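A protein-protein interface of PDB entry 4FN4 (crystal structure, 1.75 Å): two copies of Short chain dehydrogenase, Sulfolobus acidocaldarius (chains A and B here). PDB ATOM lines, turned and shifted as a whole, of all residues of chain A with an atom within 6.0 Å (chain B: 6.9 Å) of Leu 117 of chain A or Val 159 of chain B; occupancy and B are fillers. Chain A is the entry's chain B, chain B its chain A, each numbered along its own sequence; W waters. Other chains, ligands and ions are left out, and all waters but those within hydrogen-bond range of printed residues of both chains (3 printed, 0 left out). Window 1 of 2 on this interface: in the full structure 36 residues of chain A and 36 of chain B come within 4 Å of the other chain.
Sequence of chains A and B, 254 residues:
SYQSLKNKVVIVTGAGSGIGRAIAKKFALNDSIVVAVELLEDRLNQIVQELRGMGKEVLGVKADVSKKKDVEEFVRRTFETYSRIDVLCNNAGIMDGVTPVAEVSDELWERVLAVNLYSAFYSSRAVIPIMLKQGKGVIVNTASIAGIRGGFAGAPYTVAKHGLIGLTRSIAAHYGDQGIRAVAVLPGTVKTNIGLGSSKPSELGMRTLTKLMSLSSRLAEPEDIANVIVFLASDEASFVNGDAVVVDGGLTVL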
ATOM      1  N   VAL A 112     -24.456   7.530  -3.178  1.00  0.00           N
ATOM      2  CA  VAL A 112     -23.240   7.625  -3.973  1.00  0.00           C
ATOM      3  C   VAL A 112     -22.945   9.084  -4.310  1.00  0.00           C
ATOM      4  O   VAL A 112     -21.808   9.520  -4.214  1.00  0.00           O
ATOM      5  CB  VAL A 112     -23.346   6.776  -5.263  1.00  0.00           C
ATOM      6  CG1 VAL A 112     -22.129   7.026  -6.169  1.00  0.00           C
ATOM      7  CG2 VAL A 112     -23.407   5.291  -4.881  1.00  0.00           C
ATOM      8  N   LEU A 113     -23.963   9.851  -4.682  1.00  0.00           N
ATOM      9  CA  LEU A 113     -23.720  11.260  -4.991  1.00  0.00           C
ATOM     10  C   LEU A 113     -23.262  12.006  -3.739  1.00  0.00           C
ATOM     11  O   LEU A 113     -22.387  12.865  -3.802  1.00  0.00           O
ATOM     12  CB  LEU A 113     -24.986  11.913  -5.557  1.00  0.00           C
ATOM     13  CG  LEU A 113     -25.218  11.665  -7.046  1.00  0.00           C
ATOM     14  CD1 LEU A 113     -26.591  12.185  -7.450  1.00  0.00           C
ATOM     15  CD2 LEU A 113     -24.133  12.357  -7.839  1.00  0.00           C
ATOM     16  N   ALA A 114     -23.844  11.665  -2.594  1.00  0.00           N
ATOM     17  CA  ALA A 114     -23.477  12.335  -1.351  1.00  0.00           C
ATOM     18  C   ALA A 114     -22.021  12.081  -0.963  1.00  0.00           C
ATOM     19  O   ALA A 114     -21.287  13.011  -0.666  1.00  0.00           O
ATOM     20  CB  ALA A 114     -24.410  11.888  -0.211  1.00  0.00           C
ATOM     21  N   VAL A 115     -21.610  10.816  -0.954  1.00  0.00           N
ATOM     22  CA  VAL A 115     -20.243  10.466  -0.584  1.00  0.00           C
ATOM     23  C   VAL A 115     -19.189  10.843  -1.622  1.00  0.00           C
ATOM     24  O   VAL A 115     -18.113  11.317  -1.269  1.00  0.00           O
ATOM     25  CB  VAL A 115     -20.120   8.940  -0.308  1.00  0.00           C
ATOM     26  CG1 VAL A 115     -18.656   8.565  -0.022  1.00  0.00           C
ATOM     27  CG2 VAL A 115     -21.007   8.556   0.873  1.00  0.00           C
ATOM     28  N   ASN A 116     -19.498  10.650  -2.900  1.00  0.00           N
ATOM     29  CA  ASN A 116     -18.520  10.922  -3.955  1.00  0.00           C
ATOM     30  C   ASN A 116     -18.491  12.328  -4.533  1.00  0.00           C
ATOM     31  O   ASN A 116     -17.475  12.730  -5.100  1.00  0.00           O
ATOM     32  CB  ASN A 116     -18.701   9.917  -5.097  1.00  0.00           C
ATOM     33  CG  ASN A 116     -18.430   8.483  -4.661  1.00  0.00           C
ATOM     34  OD1 ASN A 116     -18.305   8.200  -3.468  1.00  0.00           O
ATOM     35  ND2 ASN A 116     -18.342   7.568  -5.630  1.00  0.00           N
ATOM     36  N   LEU A 117     -19.576  13.079  -4.372  1.00  0.00           N
ATOM     37  CA  LEU A 117     -19.645  14.427  -4.923  1.00  0.00           C
ATOM     38  C   LEU A 117     -19.994  15.530  -3.917  1.00  0.00           C
ATOM     39  O   LEU A 117     -19.264  16.512  -3.811  1.00  0.00           O
ATOM     40  CB  LEU A 117     -20.647  14.452  -6.083  1.00  0.00           C
ATOM     41  CG  LEU A 117     -20.894  15.813  -6.741  1.00  0.00           C
ATOM     42  CD1 LEU A 117     -19.588  16.359  -7.320  1.00  0.00           C
ATOM     43  CD2 LEU A 117     -21.944  15.671  -7.827  1.00  0.00           C
ATOM     44  N   TYR A 118     -21.109  15.390  -3.197  1.00  0.00           N
ATOM     45  CA  TYR A 118     -21.492  16.419  -2.224  1.00  0.00           C
ATOM     46  C   TYR A 118     -20.363  16.658  -1.219  1.00  0.00           C
ATOM     47  O   TYR A 118     -20.094  17.795  -0.828  1.00  0.00           O
ATOM     48  CB  TYR A 118     -22.764  16.025  -1.465  1.00  0.00           C
ATOM     49  CG  TYR A 118     -24.070  16.270  -2.200  1.00  0.00           C
ATOM     50  CD1 TYR A 118     -25.133  16.910  -1.556  1.00  0.00           C
ATOM     51  CD2 TYR A 118     -24.254  15.852  -3.517  1.00  0.00           C
ATOM     52  CE1 TYR A 118     -26.350  17.132  -2.203  1.00  0.00           C
ATOM     53  CE2 TYR A 118     -25.480  16.061  -4.182  1.00  0.00           C
ATOM     54  CZ  TYR A 118     -26.521  16.706  -3.514  1.00  0.00           C
ATOM     55  OH  TYR A 118     -27.729  16.942  -4.143  1.00  0.00           O
ATOM     56  N   SER A 119     -19.703  15.581  -0.815  1.00  0.00           N
ATOM     57  CA  SER A 119     -18.585  15.653   0.130  1.00  0.00           C
ATOM     58  C   SER A 119     -17.535  16.683  -0.314  1.00  0.00           C
ATOM     59  O   SER A 119     -17.080  17.503   0.488  1.00  0.00           O
ATOM     60  CB  SER A 119     -17.927  14.281   0.249  1.00  0.00           C
ATOM     61  OG  SER A 119     -17.443  13.838  -1.018  1.00  0.00           O
ATOM     62  N   ALA A 120     -17.156  16.628  -1.587  1.00  0.00           N
ATOM     63  CA  ALA A 120     -16.157  17.536  -2.140  1.00  0.00           C
ATOM     64  C   ALA A 120     -16.687  18.954  -2.283  1.00  0.00           C
ATOM     65  O   ALA A 120     -15.922  19.918  -2.207  1.00  0.00           O
ATOM     66  CB  ALA A 120     -15.653  17.014  -3.496  1.00  0.00           C
ATOM     67  N   PHE A 121     -17.991  19.093  -2.510  1.00  0.00           N
ATOM     68  CA  PHE A 121     -18.578  20.428  -2.609  1.00  0.00           C
ATOM     69  C   PHE A 121     -18.556  21.051  -1.209  1.00  0.00           C
ATOM     70  O   PHE A 121     -18.191  22.218  -1.047  1.00  0.00           O
ATOM     71  CB  PHE A 121     -20.022  20.353  -3.109  1.00  0.00           C
ATOM     72  CG  PHE A 121     -20.816  21.605  -2.841  1.00  0.00           C
ATOM     73  CD1 PHE A 121     -20.454  22.817  -3.433  1.00  0.00           C
ATOM     74  CD2 PHE A 121     -21.903  21.575  -1.969  1.00  0.00           C
ATOM     75  CE1 PHE A 121     -21.168  23.998  -3.152  1.00  0.00           C
ATOM     76  CE2 PHE A 121     -22.628  22.743  -1.677  1.00  0.00           C
ATOM     77  CZ  PHE A 121     -22.261  23.953  -2.267  1.00  0.00           C
ATOM     78  N   TYR A 122     -18.950  20.274  -0.199  1.00  0.00           N
ATOM     79  CA  TYR A 122     -18.964  20.781   1.182  1.00  0.00           C
ATOM     80  C   TYR A 122     -17.576  21.224   1.641  1.00  0.00           C
ATOM     81  O   TYR A 122     -17.404  22.311   2.205  1.00  0.00           O
ATOM     82  CB  TYR A 122     -19.448  19.707   2.155  1.00  0.00           C
ATOM     83  CG  TYR A 122     -20.875  19.237   1.969  1.00  0.00           C
ATOM     84  CD1 TYR A 122     -21.234  17.932   2.307  1.00  0.00           C
ATOM     85  CD2 TYR A 122     -21.865  20.092   1.494  1.00  0.00           C
ATOM     86  CE1 TYR A 122     -22.545  17.485   2.177  1.00  0.00           C
ATOM     87  CE2 TYR A 122     -23.188  19.655   1.362  1.00  0.00           C
ATOM     88  CZ  TYR A 122     -23.511  18.349   1.708  1.00  0.00           C
ATOM     89  OH  TYR A 122     -24.804  17.898   1.591  1.00  0.00           O
ATOM     90  N   VAL A 159     -21.961   9.246 -12.850  1.00  0.00           N
ATOM     91  CA  VAL A 159     -22.476  10.609 -12.782  1.00  0.00           C
ATOM     92  C   VAL A 159     -21.728  11.426 -11.728  1.00  0.00           C
ATOM     93  O   VAL A 159     -21.315  12.565 -11.983  1.00  0.00           O
ATOM     94  CB  VAL A 159     -23.981  10.600 -12.465  1.00  0.00           C
ATOM     95  CG1 VAL A 159     -24.457  12.007 -12.139  1.00  0.00           C
ATOM     96  CG2 VAL A 159     -24.750  10.042 -13.680  1.00  0.00           C
ATOM     97  N   ALA A 160     -21.534  10.851 -10.544  1.00  0.00           N
ATOM     98  CA  ALA A 160     -20.827  11.573  -9.487  1.00  0.00           C
ATOM     99  C   ALA A 160     -19.390  11.934  -9.877  1.00  0.00           C
ATOM    100  O   ALA A 160     -18.917  13.030  -9.568  1.00  0.00           O
ATOM    101  CB  ALA A 160     -20.823  10.741  -8.181  1.00  0.00           C
ATOM    102  N   LYS A 161     -18.696  11.023 -10.555  1.00  0.00           N
ATOM    103  CA  LYS A 161     -17.316  11.283 -10.945  1.00  0.00           C
ATOM    104  C   LYS A 161     -17.240  12.311 -12.078  1.00  0.00           C
ATOM    105  O   LYS A 161     -16.283  13.088 -12.146  1.00  0.00           O
ATOM    106  CB  LYS A 161     -16.603   9.974 -11.337  1.00  0.00           C
ATOM    107  CG  LYS A 161     -16.366   9.004 -10.155  1.00  0.00           C
ATOM    108  CD  LYS A 161     -15.470   9.604  -9.064  1.00  0.00           C
ATOM    109  CE  LYS A 161     -15.073   8.526  -8.036  1.00  0.00           C
ATOM    110  NZ  LYS A 161     -14.206   9.039  -6.933  1.00  0.00           N
ATOM    111  N   HIS A 162     -18.226  12.315 -12.974  1.00  0.00           N
ATOM    112  CA  HIS A 162     -18.251  13.328 -14.031  1.00  0.00           C
ATOM    113  C   HIS A 162     -18.485  14.656 -13.317  1.00  0.00           C
ATOM    114  O   HIS A 162     -17.868  15.666 -13.624  1.00  0.00           O
ATOM    115  CB  HIS A 162     -19.414  13.100 -15.011  1.00  0.00           C
ATOM    116  CG  HIS A 162     -19.069  12.223 -16.177  1.00  0.00           C
ATOM    117  ND1 HIS A 162     -18.843  10.868 -16.055  1.00  0.00           N
ATOM    118  CD2 HIS A 162     -18.918  12.515 -17.494  1.00  0.00           C
ATOM    119  CE1 HIS A 162     -18.568  10.363 -17.247  1.00  0.00           C
ATOM    120  NE2 HIS A 162     -18.605  11.341 -18.136  1.00  0.00           N
ATOM    121  N   GLY A 163     -19.415  14.646 -12.370  1.00  0.00           N
ATOM    122  CA  GLY A 163     -19.717  15.868 -11.639  1.00  0.00           C
ATOM    123  C   GLY A 163     -18.530  16.378 -10.841  1.00  0.00           C
ATOM    124  O   GLY A 163     -18.347  17.597 -10.696  1.00  0.00           O
ATOM    125  N   LEU A 164     -17.727  15.454 -10.317  1.00  0.00           N
ATOM    126  CA  LEU A 164     -16.554  15.826  -9.530  1.00  0.00           C
ATOM    127  C   LEU A 164     -15.520  16.521 -10.433  1.00  0.00           C
ATOM    128  O   LEU A 164     -14.842  17.449 -10.009  1.00  0.00           O
ATOM    129  CB  LEU A 164     -15.945  14.585  -8.857  1.00  0.00           C
ATOM    130  CG  LEU A 164     -14.780  14.842  -7.887  1.00  0.00           C
ATOM    131  CD1 LEU A 164     -15.242  15.746  -6.734  1.00  0.00           C
ATOM    132  CD2 LEU A 164     -14.280  13.515  -7.342  1.00  0.00           C
ATOM    133  N   GLY A 166     -16.367  18.218 -12.993  1.00  0.00           N
ATOM    134  CA  GLY A 166     -16.996  19.499 -13.243  1.00  0.00           C
ATOM    135  C   GLY A 166     -16.699  20.468 -12.110  1.00  0.00           C
ATOM    136  O   GLY A 166     -16.398  21.635 -12.350  1.00  0.00           O
ATOM    137  N   LEU A 167     -16.780  19.983 -10.872  1.00  0.00           N
ATOM    138  CA  LEU A 167     -16.511  20.827  -9.705  1.00  0.00           C
ATOM    139  C   LEU A 167     -15.060  21.302  -9.752  1.00  0.00           C
ATOM    140  O   LEU A 167     -14.754  22.456  -9.432  1.00  0.00           O
ATOM    141  CB  LEU A 167     -16.751  20.037  -8.414  1.00  0.00           C
ATOM    142  CG  LEU A 167     -16.452  20.763  -7.096  1.00  0.00           C
ATOM    143  CD1 LEU A 167     -17.509  21.855  -6.867  1.00  0.00           C
ATOM    144  CD2 LEU A 167     -16.464  19.762  -5.942  1.00  0.00           C
ATOM    145  N   SER A 170     -14.637  24.001 -12.328  1.00  0.00           N
ATOM    146  CA  SER A 170     -15.317  25.206 -11.854  1.00  0.00           C
ATOM    147  C   SER A 170     -14.428  25.981 -10.880  1.00  0.00           C
ATOM    148  O   SER A 170     -14.270  27.202 -10.993  1.00  0.00           O
ATOM    149  CB  SER A 170     -16.621  24.817 -11.158  1.00  0.00           C
ATOM    150  OG  SER A 170     -17.299  25.966 -10.694  1.00  0.00           O
ATOM    151  N   ASP B  96     -27.718  29.312 -12.616  1.00  0.00           N
ATOM    152  CA  ASP B  96     -27.382  29.372 -11.200  1.00  0.00           C
ATOM    153  C   ASP B  96     -26.790  30.673 -10.684  1.00  0.00           C
ATOM    154  O   ASP B  96     -26.095  30.668  -9.661  1.00  0.00           O
ATOM    155  CB  ASP B  96     -26.400  28.240 -10.891  1.00  0.00           C
ATOM    156  CG  ASP B  96     -25.103  28.388 -11.657  1.00  0.00           C
ATOM    157  OD1 ASP B  96     -24.972  29.372 -12.426  1.00  0.00           O
ATOM    158  OD2 ASP B  96     -24.210  27.529 -11.491  1.00  0.00           O
ATOM    159  N   VAL B 101     -18.314  28.238  -6.265  1.00  0.00           N
ATOM    160  CA  VAL B 101     -18.394  27.376  -5.077  1.00  0.00           C
ATOM    161  C   VAL B 101     -18.538  28.013  -3.690  1.00  0.00           C
ATOM    162  O   VAL B 101     -19.449  27.655  -2.935  1.00  0.00           O
ATOM    163  CB  VAL B 101     -17.193  26.396  -5.005  1.00  0.00           C
ATOM    164  CG1 VAL B 101     -17.256  25.579  -3.697  1.00  0.00           C
ATOM    165  CG2 VAL B 101     -17.220  25.440  -6.201  1.00  0.00           C
ATOM    166  N   TRP B 109     -27.481  24.848  -4.515  1.00  0.00           N
ATOM    167  CA  TRP B 109     -26.844  23.602  -4.927  1.00  0.00           C
ATOM    168  C   TRP B 109     -27.885  22.516  -5.182  1.00  0.00           C
ATOM    169  O   TRP B 109     -27.907  21.880  -6.242  1.00  0.00           O
ATOM    170  CB  TRP B 109     -25.866  23.157  -3.837  1.00  0.00           C
ATOM    171  CG  TRP B 109     -25.183  21.847  -4.076  1.00  0.00           C
ATOM    172  CD1 TRP B 109     -25.435  20.663  -3.445  1.00  0.00           C
ATOM    173  CD2 TRP B 109     -24.069  21.611  -4.943  1.00  0.00           C
ATOM    174  NE1 TRP B 109     -24.538  19.702  -3.859  1.00  0.00           N
ATOM    175  CE2 TRP B 109     -23.690  20.259  -4.780  1.00  0.00           C
ATOM    176  CE3 TRP B 109     -23.351  22.414  -5.837  1.00  0.00           C
ATOM    177  CZ2 TRP B 109     -22.624  19.692  -5.479  1.00  0.00           C
ATOM    178  CZ3 TRP B 109     -22.289  21.851  -6.529  1.00  0.00           C
ATOM    179  CH2 TRP B 109     -21.939  20.500  -6.344  1.00  0.00           C
ATOM    180  N   LEU B 113     -29.065  21.162  -9.050  1.00  0.00           N
ATOM    181  CA  LEU B 113     -28.800  19.755  -9.335  1.00  0.00           C
ATOM    182  C   LEU B 113     -30.105  18.999  -9.571  1.00  0.00           C
ATOM    183  O   LEU B 113     -30.181  18.134 -10.443  1.00  0.00           O
ATOM    184  CB  LEU B 113     -28.025  19.101  -8.190  1.00  0.00           C
ATOM    185  CG  LEU B 113     -26.533  19.433  -8.124  1.00  0.00           C
ATOM    186  CD1 LEU B 113     -25.897  18.741  -6.935  1.00  0.00           C
ATOM    187  CD2 LEU B 113     -25.868  18.992  -9.420  1.00  0.00           C
ATOM    188  N   LEU B 117     -30.181  17.923 -13.319  1.00  0.00           N
ATOM    189  CA  LEU B 117     -29.625  16.571 -13.363  1.00  0.00           C
ATOM    190  C   LEU B 117     -30.556  15.473 -12.859  1.00  0.00           C
ATOM    191  O   LEU B 117     -30.807  14.489 -13.556  1.00  0.00           O
ATOM    192  CB  LEU B 117     -28.323  16.527 -12.556  1.00  0.00           C
ATOM    193  CG  LEU B 117     -27.642  15.160 -12.424  1.00  0.00           C
ATOM    194  CD1 LEU B 117     -27.380  14.578 -13.821  1.00  0.00           C
ATOM    195  CD2 LEU B 117     -26.337  15.318 -11.651  1.00  0.00           C
ATOM    196  N   TYR B 118     -31.063  15.626 -11.641  1.00  0.00           N
ATOM    197  CA  TYR B 118     -31.930  14.589 -11.095  1.00  0.00           C
ATOM    198  C   TYR B 118     -33.155  14.371 -11.972  1.00  0.00           C
ATOM    199  O   TYR B 118     -33.604  13.240 -12.154  1.00  0.00           O
ATOM    200  CB  TYR B 118     -32.307  14.946  -9.650  1.00  0.00           C
ATOM    201  CG  TYR B 118     -31.077  15.111  -8.772  1.00  0.00           C
ATOM    202  CD1 TYR B 118     -31.146  15.766  -7.544  1.00  0.00           C
ATOM    203  CD2 TYR B 118     -29.834  14.627  -9.182  1.00  0.00           C
ATOM    204  CE1 TYR B 118     -30.000  15.935  -6.752  1.00  0.00           C
ATOM    205  CE2 TYR B 118     -28.693  14.791  -8.399  1.00  0.00           C
ATOM    206  CZ  TYR B 118     -28.779  15.445  -7.187  1.00  0.00           C
ATOM    207  OH  TYR B 118     -27.634  15.610  -6.408  1.00  0.00           O
ATOM    208  N   ALA B 146     -20.986  24.075 -20.579  1.00  0.00           N
ATOM    209  CA  ALA B 146     -20.597  24.142 -19.165  1.00  0.00           C
ATOM    210  C   ALA B 146     -20.409  22.713 -18.667  1.00  0.00           C
ATOM    211  O   ALA B 146     -19.986  22.489 -17.533  1.00  0.00           O
ATOM    212  CB  ALA B 146     -21.682  24.839 -18.329  1.00  0.00           C
ATOM    213  N   GLY B 147     -20.734  21.749 -19.527  1.00  0.00           N
ATOM    214  CA  GLY B 147     -20.571  20.352 -19.171  1.00  0.00           C
ATOM    215  C   GLY B 147     -19.182  19.846 -19.524  1.00  0.00           C
ATOM    216  O   GLY B 147     -18.834  18.698 -19.214  1.00  0.00           O
ATOM    217  N   GLY B 154     -22.029  29.011 -13.078  1.00  0.00           N
ATOM    218  CA  GLY B 154     -21.607  28.852 -11.702  1.00  0.00           C
ATOM    219  C   GLY B 154     -21.251  27.405 -11.438  1.00  0.00           C
ATOM    220  O   GLY B 154     -21.343  26.569 -12.333  1.00  0.00           O
ATOM    221  N   ALA B 155     -20.847  27.091 -10.213  1.00  0.00           N
ATOM    222  CA  ALA B 155     -20.488  25.713  -9.897  1.00  0.00           C
ATOM    223  C   ALA B 155     -21.661  24.732  -9.981  1.00  0.00           C
ATOM    224  O   ALA B 155     -21.525  23.651 -10.554  1.00  0.00           O
ATOM    225  CB  ALA B 155     -19.834  25.642  -8.514  1.00  0.00           C
ATOM    226  N   PRO B 156     -22.828  25.084  -9.416  1.00  0.00           N
ATOM    227  CA  PRO B 156     -23.966  24.152  -9.483  1.00  0.00           C
ATOM    228  C   PRO B 156     -24.315  23.727 -10.923  1.00  0.00           C
ATOM    229  O   PRO B 156     -24.493  22.541 -11.218  1.00  0.00           O
ATOM    230  CB  PRO B 156     -25.106  24.945  -8.824  1.00  0.00           C
ATOM    231  CG  PRO B 156     -24.381  25.850  -7.863  1.00  0.00           C
ATOM    232  CD  PRO B 156     -23.184  26.305  -8.669  1.00  0.00           C
ATOM    233  N   TYR B 157     -24.406  24.703 -11.814  1.00  0.00           N
ATOM    234  CA  TYR B 157     -24.752  24.442 -13.211  1.00  0.00           C
ATOM    235  C   TYR B 157     -23.659  23.620 -13.897  1.00  0.00           C
ATOM    236  O   TYR B 157     -23.937  22.652 -14.605  1.00  0.00           O
ATOM    237  CB  TYR B 157     -24.934  25.774 -13.943  1.00  0.00           C
ATOM    238  CG  TYR B 157     -25.552  25.686 -15.322  1.00  0.00           C
ATOM    239  CD1 TYR B 157     -26.941  25.760 -15.495  1.00  0.00           C
ATOM    240  CD2 TYR B 157     -24.747  25.655 -16.459  1.00  0.00           C
ATOM    241  CE1 TYR B 157     -27.503  25.822 -16.769  1.00  0.00           C
ATOM    242  CE2 TYR B 157     -25.299  25.721 -17.741  1.00  0.00           C
ATOM    243  CZ  TYR B 157     -26.671  25.812 -17.889  1.00  0.00           C
ATOM    244  OH  TYR B 157     -27.193  25.958 -19.159  1.00  0.00           O
ATOM    245  N   THR B 158     -22.410  24.004 -13.679  1.00  0.00           N
ATOM    246  CA  THR B 158     -21.292  23.286 -14.285  1.00  0.00           C
ATOM    247  C   THR B 158     -21.252  21.843 -13.814  1.00  0.00           C
ATOM    248  O   THR B 158     -21.077  20.913 -14.608  1.00  0.00           O
ATOM    249  CB  THR B 158     -19.990  24.006 -13.944  1.00  0.00           C
ATOM    250  OG1 THR B 158     -20.051  25.317 -14.513  1.00  0.00           O
ATOM    251  CG2 THR B 158     -18.777  23.276 -14.507  1.00  0.00           C
ATOM    252  N   VAL B 159     -21.446  21.648 -12.515  1.00  0.00           N
ATOM    253  CA  VAL B 159     -21.442  20.302 -11.969  1.00  0.00           C
ATOM    254  C   VAL B 159     -22.619  19.499 -12.512  1.00  0.00           C
ATOM    255  O   VAL B 159     -22.460  18.344 -12.901  1.00  0.00           O
ATOM    256  CB  VAL B 159     -21.517  20.344 -10.436  1.00  0.00           C
ATOM    257  CG1 VAL B 159     -21.757  18.929  -9.877  1.00  0.00           C
ATOM    258  CG2 VAL B 159     -20.200  20.888  -9.890  1.00  0.00           C
ATOM    259  N   ALA B 160     -23.798  20.110 -12.550  1.00  0.00           N
ATOM    260  CA  ALA B 160     -24.976  19.405 -13.044  1.00  0.00           C
ATOM    261  C   ALA B 160     -24.833  18.997 -14.504  1.00  0.00           C
ATOM    262  O   ALA B 160     -25.185  17.871 -14.877  1.00  0.00           O
ATOM    263  CB  ALA B 160     -26.226  20.270 -12.871  1.00  0.00           C
ATOM    264  N   LYS B 161     -24.323  19.907 -15.329  1.00  0.00           N
ATOM    265  CA  LYS B 161     -24.165  19.620 -16.751  1.00  0.00           C
ATOM    266  C   LYS B 161     -23.082  18.570 -17.008  1.00  0.00           C
ATOM    267  O   LYS B 161     -23.212  17.782 -17.942  1.00  0.00           O
ATOM    268  CB  LYS B 161     -23.892  20.912 -17.523  1.00  0.00           C
ATOM    269  CG  LYS B 161     -25.077  21.901 -17.517  1.00  0.00           C
ATOM    270  CD  LYS B 161     -26.338  21.314 -18.181  1.00  0.00           C
ATOM    271  CE  LYS B 161     -27.412  22.385 -18.384  1.00  0.00           C
ATOM    272  NZ  LYS B 161     -28.644  21.864 -19.066  1.00  0.00           N
ATOM    273  N   HIS B 162     -22.022  18.557 -16.196  1.00  0.00           N
ATOM    274  CA  HIS B 162     -20.992  17.527 -16.348  1.00  0.00           C
ATOM    275  C   HIS B 162     -21.653  16.202 -15.976  1.00  0.00           C
ATOM    276  O   HIS B 162     -21.471  15.192 -16.644  1.00  0.00           O
ATOM    277  CB  HIS B 162     -19.809  17.753 -15.391  1.00  0.00           C
ATOM    278  CG  HIS B 162     -18.737  18.635 -15.946  1.00  0.00           C
ATOM    279  ND1 HIS B 162     -18.903  19.991 -16.135  1.00  0.00           N
ATOM    280  CD2 HIS B 162     -17.478  18.350 -16.355  1.00  0.00           C
ATOM    281  CE1 HIS B 162     -17.792  20.503 -16.636  1.00  0.00           C
ATOM    282  NE2 HIS B 162     -16.912  19.529 -16.779  1.00  0.00           N
ATOM    283  N   GLY B 163     -22.417  16.221 -14.885  1.00  0.00           N
ATOM    284  CA  GLY B 163     -23.097  15.016 -14.445  1.00  0.00           C
ATOM    285  C   GLY B 163     -24.077  14.505 -15.490  1.00  0.00           C
ATOM    286  O   GLY B 163     -24.224  13.289 -15.669  1.00  0.00           O
ATOM    287  N   LEU B 164     -24.733  15.427 -16.194  1.00  0.00           N
ATOM    288  CA  LEU B 164     -25.711  15.049 -17.218  1.00  0.00           C
ATOM    289  C   LEU B 164     -25.029  14.348 -18.407  1.00  0.00           C
ATOM    290  O   LEU B 164     -25.590  13.420 -19.001  1.00  0.00           O
ATOM    291  CB  LEU B 164     -26.491  16.284 -17.683  1.00  0.00           C
ATOM    292  CG  LEU B 164     -27.645  16.026 -18.654  1.00  0.00           C
ATOM    293  CD1 LEU B 164     -28.705  15.180 -17.969  1.00  0.00           C
ATOM    294  CD2 LEU B 164     -28.248  17.362 -19.099  1.00  0.00           C
HETATM  295  O   HOH W   1     -18.208  26.921 -13.066  1.00  0.00           O
HETATM  296  O   HOH W   2     -28.672  13.707  -4.669  1.00  0.00           O
HETATM  297  O   HOH W   3     -16.647  27.769  -8.492  1.00  0.00           O
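The side-chain hydroxyl (OH) of Tyr 118 of chain B sits at hydrogen-bond distance from the side-chain hydroxyl (OH) of Tyr 118 of chain A (2.6 Å).
O of Leu 113 of chain B sits at hydrogen-bond distance from N of Tyr 118 of chain B. The backbone carbonyl oxygen of Ala 146 of chain B sits at hydrogen-bond distance from a ring nitrogen (ND1) of His 162 of chain B. The backbone carbonyl oxygen of Gly 147 of chain B sits close to a ring nitrogen (NE2) of His 162 of chain B (3.2 Å). O of Thr 158 of chain B lies within hydrogen-bond range of ND1 of His 162 of chain B (2.8 Å). The backbone carbonyl oxygen (O) of Leu 113 of chain A is in hydrogen-bond range of the backbone NH (N) of Tyr 118 of chain A, at 2.9 Å.
Among the printed residues, merely in contact across the chains: Leu 113 of chain A with Tyr 118 of chain B, Leu 117 of chain A with Val 159 of chain B, Tyr 118 of chain A with Trp 109 of chain B, Tyr 118 of chain A with Leu 113 of chain B, Phe 121 of chain A with Trp 109 of chain B, Val 159 of chain A with Leu 117 of chain B, Val 159 of chain A with Gly 163 of chain B, His 162 of chain A with His 162 of chain B, Gly 163 of chain A with Val 159 of chain B, Gly 166 of chain A with Thr 158 of chain B, Gly 166 of chain A with His 162 of chain B, Leu 167 of chain A with Val 101 of chain B, Leu 167 of chain A with Val 159 of chain B and Ser 170 of chain A with Ala 155 of chain B.
Of chain B, only Val 159 (3.9 Å) comes within 4 Å of Leu 117 of chain A. Printed residues of chain B within 4 Å of Phe 121 of chain A: Trp 109. Of the printed residues of chain A, Trp 109 of chain B touches Tyr 118 and Phe 121. Val 159 of chain B touches just these residues of chain A: Leu 117 (3.9 Å), Gly 163 (3.8 Å) and Leu 167 (3.7 Å). The nearest residue of chain A that does not touch Val 159 of chain B is Gly 166 of chain A (4.2 Å).
Hydrophobic or aromatic side chains of chain A that line the printed part of chain B: Leu 113, Leu 117, Tyr 118, Phe 121, Val 159, His 162 and Leu 167. Of the 19 printed residues of chain B, 10 touch a printed residue of chain A. Printed residues of chain B that touch a printed residue of chain A: Val 101, Trp 109, Leu 113, Leu 117, Tyr 118, Ala 155, Thr 158, Val 159, His 162 and Gly 163. Along chain B the printed residues that touch a printed residue of chain A span positions 101 to 163. Among the printed residues, no Asp or Glu carboxylate lies within 4 Å of a Lys or Arg side-chain nitrogen of the other chain.
Leu 117 of chain A touches Val 159 of chain B, and with the chains exchanged Val 159 of chain A touches Leu 117 of chain B. Tyr 118 of chain B touches its own counterpart, Tyr 118 of chain A. Val 159 of chain A touches Gly 163 of chain B, and with the chains exchanged Gly 163 of chain A touches Val 159 of chain B. His 162 of chain A touches its own counterpart, His 162 of chain B. Of the 15 pairs that touch across the chains among the printed residues, 8 have their exchanged pair printed and touching as well.
Water W1 lies within hydrogen-bond range of OG of Ser 170 of chain A (2.7 Å), OG1 of Thr 158 of chain B (2.8 Å) and O of Gly 154 of chain B (3.2 Å). Water W2 bridges OH of Tyr 118 of chain B and OH of Tyr 118 of chain A. Water W3 bridges the backbone NH (N) of Val 101 of chain B and the side-chain hydroxyl (OG) of Ser 170 of chain A.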
